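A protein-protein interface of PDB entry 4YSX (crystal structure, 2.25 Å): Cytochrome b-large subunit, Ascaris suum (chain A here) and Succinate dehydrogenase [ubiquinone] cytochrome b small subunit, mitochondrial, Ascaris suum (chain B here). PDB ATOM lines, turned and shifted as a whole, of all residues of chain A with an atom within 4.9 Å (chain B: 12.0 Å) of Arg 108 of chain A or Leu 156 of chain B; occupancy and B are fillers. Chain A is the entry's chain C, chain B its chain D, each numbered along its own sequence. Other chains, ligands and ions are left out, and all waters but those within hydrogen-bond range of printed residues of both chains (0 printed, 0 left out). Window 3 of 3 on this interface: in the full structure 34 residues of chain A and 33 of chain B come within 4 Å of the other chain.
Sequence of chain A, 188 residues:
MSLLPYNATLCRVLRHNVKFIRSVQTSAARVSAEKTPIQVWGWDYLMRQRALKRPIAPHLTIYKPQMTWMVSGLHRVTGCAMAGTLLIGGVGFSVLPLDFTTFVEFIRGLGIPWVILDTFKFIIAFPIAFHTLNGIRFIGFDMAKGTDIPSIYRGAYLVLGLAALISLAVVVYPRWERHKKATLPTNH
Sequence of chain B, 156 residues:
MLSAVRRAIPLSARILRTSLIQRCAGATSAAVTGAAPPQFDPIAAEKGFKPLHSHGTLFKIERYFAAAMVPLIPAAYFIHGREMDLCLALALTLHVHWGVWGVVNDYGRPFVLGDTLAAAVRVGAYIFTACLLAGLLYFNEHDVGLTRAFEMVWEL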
ATOM      1  N   VAL A 104      21.952 -18.045  25.349  1.00  0.00           N
ATOM      2  CA  VAL A 104      21.135 -17.364  24.343  1.00  0.00           C
ATOM      3  C   VAL A 104      19.735 -17.093  24.887  1.00  0.00           C
ATOM      4  O   VAL A 104      19.203 -15.995  24.712  1.00  0.00           O
ATOM      5  CB  VAL A 104      21.061 -18.155  23.014  1.00  0.00           C
ATOM      6  CG1 VAL A 104      19.961 -17.622  22.104  1.00  0.00           C
ATOM      7  CG2 VAL A 104      22.401 -18.093  22.298  1.00  0.00           C
ATOM      8  N   GLU A 105      19.150 -18.086  25.552  1.00  0.00           N
ATOM      9  CA  GLU A 105      17.793 -17.955  26.092  1.00  0.00           C
ATOM     10  C   GLU A 105      17.745 -16.852  27.161  1.00  0.00           C
ATOM     11  O   GLU A 105      16.763 -16.108  27.244  1.00  0.00           O
ATOM     12  CB  GLU A 105      17.283 -19.309  26.629  1.00  0.00           C
ATOM     13  CG  GLU A 105      15.849 -19.319  27.164  1.00  0.00           C
ATOM     14  CD  GLU A 105      14.798 -18.883  26.144  1.00  0.00           C
ATOM     15  OE1 GLU A 105      14.006 -17.970  26.466  1.00  0.00           O
ATOM     16  OE2 GLU A 105      14.757 -19.445  25.029  1.00  0.00           O
ATOM     17  N   PHE A 106      18.817 -16.720  27.946  1.00  0.00           N
ATOM     18  CA  PHE A 106      18.908 -15.641  28.933  1.00  0.00           C
ATOM     19  C   PHE A 106      18.759 -14.244  28.313  1.00  0.00           C
ATOM     20  O   PHE A 106      18.021 -13.413  28.853  1.00  0.00           O
ATOM     21  CB  PHE A 106      20.217 -15.716  29.727  1.00  0.00           C
ATOM     22  CG  PHE A 106      20.593 -14.421  30.409  1.00  0.00           C
ATOM     23  CD1 PHE A 106      19.827 -13.919  31.454  1.00  0.00           C
ATOM     24  CD2 PHE A 106      21.709 -13.702  30.001  1.00  0.00           C
ATOM     25  CE1 PHE A 106      20.164 -12.730  32.076  1.00  0.00           C
ATOM     26  CE2 PHE A 106      22.054 -12.514  30.620  1.00  0.00           C
ATOM     27  CZ  PHE A 106      21.279 -12.027  31.659  1.00  0.00           C
ATOM     28  N   ILE A 107      19.436 -13.978  27.193  1.00  0.00           N
ATOM     29  CA  ILE A 107      19.430 -12.611  26.638  1.00  0.00           C
ATOM     30  C   ILE A 107      18.128 -12.302  25.882  1.00  0.00           C
ATOM     31  O   ILE A 107      17.669 -11.157  25.884  1.00  0.00           O
ATOM     32  CB  ILE A 107      20.698 -12.243  25.803  1.00  0.00           C
ATOM     33  CG1 ILE A 107      20.486 -12.413  24.297  1.00  0.00           C
ATOM     34  CG2 ILE A 107      21.934 -13.006  26.274  1.00  0.00           C
ATOM     35  CD1 ILE A 107      21.574 -11.752  23.477  1.00  0.00           C
ATOM     36  N   ARG A 108      17.539 -13.313  25.245  1.00  0.00           N
ATOM     37  CA  ARG A 108      16.175 -13.191  24.717  1.00  0.00           C
ATOM     38  C   ARG A 108      15.222 -12.812  25.847  1.00  0.00           C
ATOM     39  O   ARG A 108      14.363 -11.949  25.671  1.00  0.00           O
ATOM     40  CB  ARG A 108      15.732 -14.494  24.052  1.00  0.00           C
ATOM     41  CG  ARG A 108      14.236 -14.603  23.775  1.00  0.00           C
ATOM     42  CD  ARG A 108      13.934 -15.104  22.369  1.00  0.00           C
ATOM     43  NE  ARG A 108      14.879 -16.124  21.910  1.00  0.00           N
ATOM     44  CZ  ARG A 108      15.128 -16.419  20.632  1.00  0.00           C
ATOM     45  NH1 ARG A 108      16.023 -17.358  20.343  1.00  0.00           N
ATOM     46  NH2 ARG A 108      14.499 -15.787  19.639  1.00  0.00           N
ATOM     47  N   GLY A 109      15.404 -13.446  27.007  1.00  0.00           N
ATOM     48  CA  GLY A 109      14.631 -13.144  28.212  1.00  0.00           C
ATOM     49  C   GLY A 109      14.642 -11.680  28.632  1.00  0.00           C
ATOM     50  O   GLY A 109      13.658 -11.187  29.185  1.00  0.00           O
ATOM     51  N   LEU A 110      15.751 -10.987  28.371  1.00  0.00           N
ATOM     52  CA  LEU A 110      15.861  -9.543  28.628  1.00  0.00           C
ATOM     53  C   LEU A 110      15.029  -8.716  27.637  1.00  0.00           C
ATOM     54  O   LEU A 110      14.803  -7.527  27.862  1.00  0.00           O
ATOM     55  CB  LEU A 110      17.326  -9.090  28.560  1.00  0.00           C
ATOM     56  CG  LEU A 110      18.329  -9.761  29.510  1.00  0.00           C
ATOM     57  CD1 LEU A 110      19.758  -9.460  29.082  1.00  0.00           C
ATOM     58  CD2 LEU A 110      18.104  -9.328  30.951  1.00  0.00           C
ATOM     59  N   GLY A 111      14.609  -9.340  26.535  1.00  0.00           N
ATOM     60  CA  GLY A 111      13.686  -8.734  25.573  1.00  0.00           C
ATOM     61  C   GLY A 111      14.067  -7.341  25.114  1.00  0.00           C
ATOM     62  O   GLY A 111      13.210  -6.467  24.989  1.00  0.00           O
ATOM     63  N   LEU A 117      19.702  -5.325  19.225  1.00  0.00           N
ATOM     64  CA  LEU A 117      20.136  -6.702  18.974  1.00  0.00           C
ATOM     65  C   LEU A 117      20.862  -6.797  17.645  1.00  0.00           C
ATOM     66  O   LEU A 117      21.943  -7.377  17.574  1.00  0.00           O
ATOM     67  CB  LEU A 117      18.958  -7.686  18.973  1.00  0.00           C
ATOM     68  CG  LEU A 117      18.355  -8.058  20.329  1.00  0.00           C
ATOM     69  CD1 LEU A 117      17.034  -8.790  20.157  1.00  0.00           C
ATOM     70  CD2 LEU A 117      19.330  -8.894  21.146  1.00  0.00           C
ATOM     71  N   ASP A 118      20.277  -6.218  16.602  1.00  0.00           N
ATOM     72  CA  ASP A 118      20.891  -6.236  15.265  1.00  0.00           C
ATOM     73  C   ASP A 118      22.172  -5.394  15.159  1.00  0.00           C
ATOM     74  O   ASP A 118      23.007  -5.631  14.280  1.00  0.00           O
ATOM     75  CB  ASP A 118      19.879  -5.802  14.201  1.00  0.00           C
ATOM     76  CG  ASP A 118      19.009  -6.958  13.718  1.00  0.00           C
ATOM     77  OD1 ASP A 118      18.533  -6.902  12.566  1.00  0.00           O
ATOM     78  OD2 ASP A 118      18.820  -7.936  14.473  1.00  0.00           O
ATOM     79  N   LYS A 121      24.845  -7.757  16.418  1.00  0.00           N
ATOM     80  CA  LYS A 121      25.182  -8.626  15.288  1.00  0.00           C
ATOM     81  C   LYS A 121      26.139  -7.933  14.319  1.00  0.00           C
ATOM     82  O   LYS A 121      27.126  -8.533  13.878  1.00  0.00           O
ATOM     83  CB  LYS A 121      23.924  -9.056  14.530  1.00  0.00           C
ATOM     84  CG  LYS A 121      22.966  -9.910  15.333  1.00  0.00           C
ATOM     85  CD  LYS A 121      21.643 -10.130  14.618  1.00  0.00           C
ATOM     86  CE  LYS A 121      20.536 -10.446  15.614  1.00  0.00           C
ATOM     87  NZ  LYS A 121      19.223 -10.698  14.962  1.00  0.00           N
ATOM     88  N   ARG A 175      16.667 -10.062   8.815  1.00  0.00           N
ATOM     89  CA  ARG A 175      15.657  -9.262   9.507  1.00  0.00           C
ATOM     90  C   ARG A 175      14.520  -8.910   8.551  1.00  0.00           C
ATOM     91  O   ARG A 175      13.373  -8.837   8.963  1.00  0.00           O
ATOM     92  CB  ARG A 175      16.246  -7.963  10.048  1.00  0.00           C
ATOM     93  CG  ARG A 175      15.386  -7.330  11.129  1.00  0.00           C
ATOM     94  CD  ARG A 175      15.796  -7.843  12.493  1.00  0.00           C
ATOM     95  NE  ARG A 175      14.681  -8.281  13.313  1.00  0.00           N
ATOM     96  CZ  ARG A 175      14.793  -8.656  14.585  1.00  0.00           C
ATOM     97  NH1 ARG A 175      15.973  -8.636  15.196  1.00  0.00           N
ATOM     98  NH2 ARG A 175      13.717  -9.051  15.253  1.00  0.00           N
ATOM     99  N   ARG A 178      12.330 -11.939   8.123  1.00  0.00           N
ATOM    100  CA  ARG A 178      11.533 -12.097   9.345  1.00  0.00           C
ATOM    101  C   ARG A 178      10.353 -11.127   9.479  1.00  0.00           C
ATOM    102  O   ARG A 178       9.365 -11.443  10.148  1.00  0.00           O
ATOM    103  CB  ARG A 178      12.415 -11.971  10.586  1.00  0.00           C
ATOM    104  CG  ARG A 178      13.125 -13.261  10.954  1.00  0.00           C
ATOM    105  CD  ARG A 178      13.279 -13.368  12.455  1.00  0.00           C
ATOM    106  NE  ARG A 178      14.465 -12.679  12.936  1.00  0.00           N
ATOM    107  CZ  ARG A 178      14.636 -12.234  14.180  1.00  0.00           C
ATOM    108  NH1 ARG A 178      13.681 -12.352  15.098  1.00  0.00           N
ATOM    109  NH2 ARG A 178      15.778 -11.648  14.508  1.00  0.00           N
ATOM    110  N   VAL B 144      27.018 -26.486  21.250  1.00  0.00           N
ATOM    111  CA  VAL B 144      26.367 -26.427  19.945  1.00  0.00           C
ATOM    112  C   VAL B 144      27.318 -26.376  18.755  1.00  0.00           C
ATOM    113  O   VAL B 144      26.923 -26.700  17.652  1.00  0.00           O
ATOM    114  CB  VAL B 144      25.381 -25.233  19.872  1.00  0.00           C
ATOM    115  CG1 VAL B 144      24.210 -25.452  20.825  1.00  0.00           C
ATOM    116  CG2 VAL B 144      26.070 -23.902  20.164  1.00  0.00           C
ATOM    117  N   THR B 147      29.309 -22.870  14.158  1.00  0.00           N
ATOM    118  CA  THR B 147      28.353 -22.450  13.125  1.00  0.00           C
ATOM    119  C   THR B 147      26.931 -22.310  13.680  1.00  0.00           C
ATOM    120  O   THR B 147      26.270 -21.306  13.443  1.00  0.00           O
ATOM    121  CB  THR B 147      28.369 -23.389  11.893  1.00  0.00           C
ATOM    122  OG1 THR B 147      28.350 -24.765  12.299  1.00  0.00           O
ATOM    123  CG2 THR B 147      29.611 -23.144  11.050  1.00  0.00           C
ATOM    124  N   ARG B 148      26.471 -23.295  14.443  1.00  0.00           N
ATOM    125  CA  ARG B 148      25.153 -23.212  15.092  1.00  0.00           C
ATOM    126  C   ARG B 148      25.092 -22.081  16.128  1.00  0.00           C
ATOM    127  O   ARG B 148      24.035 -21.478  16.313  1.00  0.00           O
ATOM    128  CB  ARG B 148      24.754 -24.582  15.707  1.00  0.00           C
ATOM    129  CG  ARG B 148      23.794 -24.554  16.894  1.00  0.00           C
ATOM    130  CD  ARG B 148      22.334 -24.909  16.618  1.00  0.00           C
ATOM    131  NE  ARG B 148      21.613 -23.953  15.784  1.00  0.00           N
ATOM    132  CZ  ARG B 148      20.329 -23.606  15.934  1.00  0.00           C
ATOM    133  NH1 ARG B 148      19.583 -24.083  16.928  1.00  0.00           N
ATOM    134  NH2 ARG B 148      19.783 -22.741  15.082  1.00  0.00           N
ATOM    135  N   ALA B 149      26.210 -21.809  16.809  1.00  0.00           N
ATOM    136  CA  ALA B 149      26.277 -20.711  17.796  1.00  0.00           C
ATOM    137  C   ALA B 149      25.923 -19.391  17.132  1.00  0.00           C
ATOM    138  O   ALA B 149      25.155 -18.598  17.668  1.00  0.00           O
ATOM    139  CB  ALA B 149      27.665 -20.617  18.422  1.00  0.00           C
ATOM    140  N   PHE B 150      26.491 -19.173  15.953  1.00  0.00           N
ATOM    141  CA  PHE B 150      26.174 -18.006  15.162  1.00  0.00           C
ATOM    142  C   PHE B 150      24.697 -17.970  14.752  1.00  0.00           C
ATOM    143  O   PHE B 150      24.067 -16.913  14.794  1.00  0.00           O
ATOM    144  CB  PHE B 150      27.053 -17.957  13.912  1.00  0.00           C
ATOM    145  CG  PHE B 150      28.399 -17.307  14.118  1.00  0.00           C
ATOM    146  CD1 PHE B 150      29.514 -18.064  14.445  1.00  0.00           C
ATOM    147  CD2 PHE B 150      28.562 -15.946  13.912  1.00  0.00           C
ATOM    148  CE1 PHE B 150      30.756 -17.476  14.603  1.00  0.00           C
ATOM    149  CE2 PHE B 150      29.800 -15.347  14.071  1.00  0.00           C
ATOM    150  CZ  PHE B 150      30.898 -16.111  14.421  1.00  0.00           C
ATOM    151  N   GLU B 151      24.146 -19.105  14.330  1.00  0.00           N
ATOM    152  CA  GLU B 151      22.720 -19.157  13.971  1.00  0.00           C
ATOM    153  C   GLU B 151      21.871 -18.678  15.137  1.00  0.00           C
ATOM    154  O   GLU B 151      20.996 -17.826  14.980  1.00  0.00           O
ATOM    155  CB  GLU B 151      22.269 -20.570  13.607  1.00  0.00           C
ATOM    156  CG  GLU B 151      22.904 -21.171  12.365  1.00  0.00           C
ATOM    157  CD  GLU B 151      22.478 -22.620  12.144  1.00  0.00           C
ATOM    158  OE1 GLU B 151      23.254 -23.388  11.524  1.00  0.00           O
ATOM    159  OE2 GLU B 151      21.367 -22.986  12.590  1.00  0.00           O
ATOM    160  N   MET B 152      22.152 -19.225  16.312  1.00  0.00           N
ATOM    161  CA  MET B 152      21.354 -18.933  17.500  1.00  0.00           C
ATOM    162  C   MET B 152      21.388 -17.460  17.912  1.00  0.00           C
ATOM    163  O   MET B 152      20.363 -16.927  18.345  1.00  0.00           O
ATOM    164  CB  MET B 152      21.758 -19.842  18.657  1.00  0.00           C
ATOM    165  CG  MET B 152      21.388 -21.303  18.409  1.00  0.00           C
ATOM    166  SD  MET B 152      22.178 -22.479  19.530  1.00  0.00           S
ATOM    167  CE  MET B 152      21.698 -21.811  21.118  1.00  0.00           C
ATOM    168  N   VAL B 153      22.534 -16.788  17.761  1.00  0.00           N
ATOM    169  CA  VAL B 153      22.575 -15.341  18.034  1.00  0.00           C
ATOM    170  C   VAL B 153      21.870 -14.542  16.932  1.00  0.00           C
ATOM    171  O   VAL B 153      21.141 -13.606  17.231  1.00  0.00           O
ATOM    172  CB  VAL B 153      24.001 -14.783  18.312  1.00  0.00           C
ATOM    173  CG1 VAL B 153      24.659 -15.520  19.469  1.00  0.00           C
ATOM    174  CG2 VAL B 153      24.880 -14.843  17.082  1.00  0.00           C
ATOM    175  N   TRP B 154      22.072 -14.923  15.673  1.00  0.00           N
ATOM    176  CA  TRP B 154      21.408 -14.252  14.557  1.00  0.00           C
ATOM    177  C   TRP B 154      19.870 -14.376  14.587  1.00  0.00           C
ATOM    178  O   TRP B 154      19.171 -13.473  14.128  1.00  0.00           O
ATOM    179  CB  TRP B 154      21.972 -14.717  13.192  1.00  0.00           C
ATOM    180  CG  TRP B 154      22.776 -13.626  12.513  1.00  0.00           C
ATOM    181  CD1 TRP B 154      22.413 -12.905  11.420  1.00  0.00           C
ATOM    182  CD2 TRP B 154      24.047 -13.096  12.935  1.00  0.00           C
ATOM    183  NE1 TRP B 154      23.382 -11.975  11.120  1.00  0.00           N
ATOM    184  CE2 TRP B 154      24.395 -12.075  12.036  1.00  0.00           C
ATOM    185  CE3 TRP B 154      24.929 -13.403  13.976  1.00  0.00           C
ATOM    186  CZ2 TRP B 154      25.590 -11.352  12.148  1.00  0.00           C
ATOM    187  CZ3 TRP B 154      26.116 -12.684  14.090  1.00  0.00           C
ATOM    188  CH2 TRP B 154      26.430 -11.667  13.184  1.00  0.00           C
ATOM    189  N   GLU B 155      19.345 -15.468  15.140  1.00  0.00           N
ATOM    190  CA  GLU B 155      17.890 -15.666  15.219  1.00  0.00           C
ATOM    191  C   GLU B 155      17.221 -14.711  16.199  1.00  0.00           C
ATOM    192  O   GLU B 155      16.053 -14.374  16.027  1.00  0.00           O
ATOM    193  CB  GLU B 155      17.547 -17.108  15.605  1.00  0.00           C
ATOM    194  CG  GLU B 155      17.646 -18.082  14.444  1.00  0.00           C
ATOM    195  CD  GLU B 155      17.594 -19.541  14.877  1.00  0.00           C
ATOM    196  OE1 GLU B 155      17.257 -19.817  16.054  1.00  0.00           O
ATOM    197  OE2 GLU B 155      17.896 -20.408  14.028  1.00  0.00           O
ATOM    198  N   LEU B 156      17.963 -14.284  17.219  1.00  0.00           N
ATOM    199  CA  LEU B 156      17.453 -13.371  18.250  1.00  0.00           C
ATOM    200  C   LEU B 156      16.620 -12.217  17.687  1.00  0.00           C
ATOM    201  O   LEU B 156      15.580 -11.843  18.232  1.00  0.00           O
ATOM    202  CB  LEU B 156      18.616 -12.776  19.037  1.00  0.00           C
ATOM    203  CG  LEU B 156      19.343 -13.705  20.004  1.00  0.00           C
ATOM    204  CD1 LEU B 156      20.673 -13.095  20.417  1.00  0.00           C
ATOM    205  CD2 LEU B 156      18.472 -13.973  21.222  1.00  0.00           C
ATOM    206  OXT LEU B 156      16.988 -11.618  16.674  1.00  0.00           O
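The guanidinium group (NH2) of Arg 178 of chain A sits at hydrogen-bond distance from the backbone carbonyl oxygen (O) of Glu 155 of chain B, at 3.1 Å. The chain-end carboxylate of Leu 156 of chain B lies within salt-bridge range of the side-chain amino group of Lys 121 of chain A (3.0 Å). NZ of Lys 121 of chain A is in hydrogen-bond range of O of Trp 154 of chain B. OXT of Leu 156 of chain B is in salt-bridge range of NH2 of Arg 178 of chain A. The guanidinium group of Arg 175 of chain A lies within salt-bridge range of the chain-end carboxylate of Leu 156 of chain B, 3.5 Å away.
Val 104 of chain A touches Met 152 of chain B. CD1 of Leu 156 of chain B touches CD1 of Ile 107 of chain A, at 3.5 Å. Arg 108 of chain A touches Leu 156 of chain B (CB to CD2, 3.97 Å). Leu 117 of chain A touches Leu 156 of chain B. Lys 121 of chain A touches Val 153 of chain B. Trp 154 of chain B touches Arg 178 of chain A (O to NH2, 3.9 Å).
Val 104 of chain A touches one residue of chain B. No residue of chain B comes within 4 Å of Phe 106 of chain A. No residue of chain B comes within 4 Å of Gly 109 of chain A. No residue of chain B comes within 4 Å of Leu 110 of chain A. Of chain B, only Leu 156 (3.9 Å) comes within 4 Å of Leu 117 of chain A. Of the printed residues of chain B, Arg 175 of chain A touches Leu 156 (3.5 Å). Printed residues of chain B within 4 Å of Arg 178 of chain A: Trp 154 (3.9 Å), Glu 155 (3.1 Å) and Leu 156 (2.5 Å). Arg 148 of chain B touches none of the printed residues of chain A. Phe 150 of chain B touches none of the printed residues of chain A. Of the printed residues of chain A, Val 153 of chain B touches Lys 121 (3.6 Å). Of the printed residues of chain A, Trp 154 of chain B touches Lys 121 (2.9 Å) and Arg 178 (3.9 Å). Of the printed residues of chain A, Glu 155 of chain B touches Arg 178. Of chain A, only Ile 107 (3.5 Å), Arg 108 (3.97 Å), Leu 117 (3.9 Å), Lys 121 (3.0 Å), Arg 175 (3.5 Å) and Arg 178 (2.5 Å) come within 4 Å of Leu 156 of chain B. The nearest residue of chain A that does not touch Leu 156 of chain B is Val 104 of chain A (4.04 Å).
Of the 13 printed residues of chain A, 7 touch a printed residue of chain B. Printed residues of chain B that touch a printed residue of chain A: Met 152, Val 153, Trp 154, Glu 155 and Leu 156. Hydrophobic or aromatic side chains of chain B that line the printed part of chain A: Met 152, Trp 154 and Leu 156. Among the printed residues, 11 pairs touch across the chains.
NH1 of Arg 175 of chain A lies within salt-bridge range of OD2 of Asp 118 of chain A, 3.0 Å away. The side-chain amino group of Lys 121 of chain A lies within salt-bridge range of the side-chain carboxylate of Asp 118 of chain A (2.8 Å). The side-chain carboxylate (OE2) of Glu 155 of chain B lies within salt-bridge range of the guanidinium group (NH2) of Arg 148 of chain B (3.2 Å).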
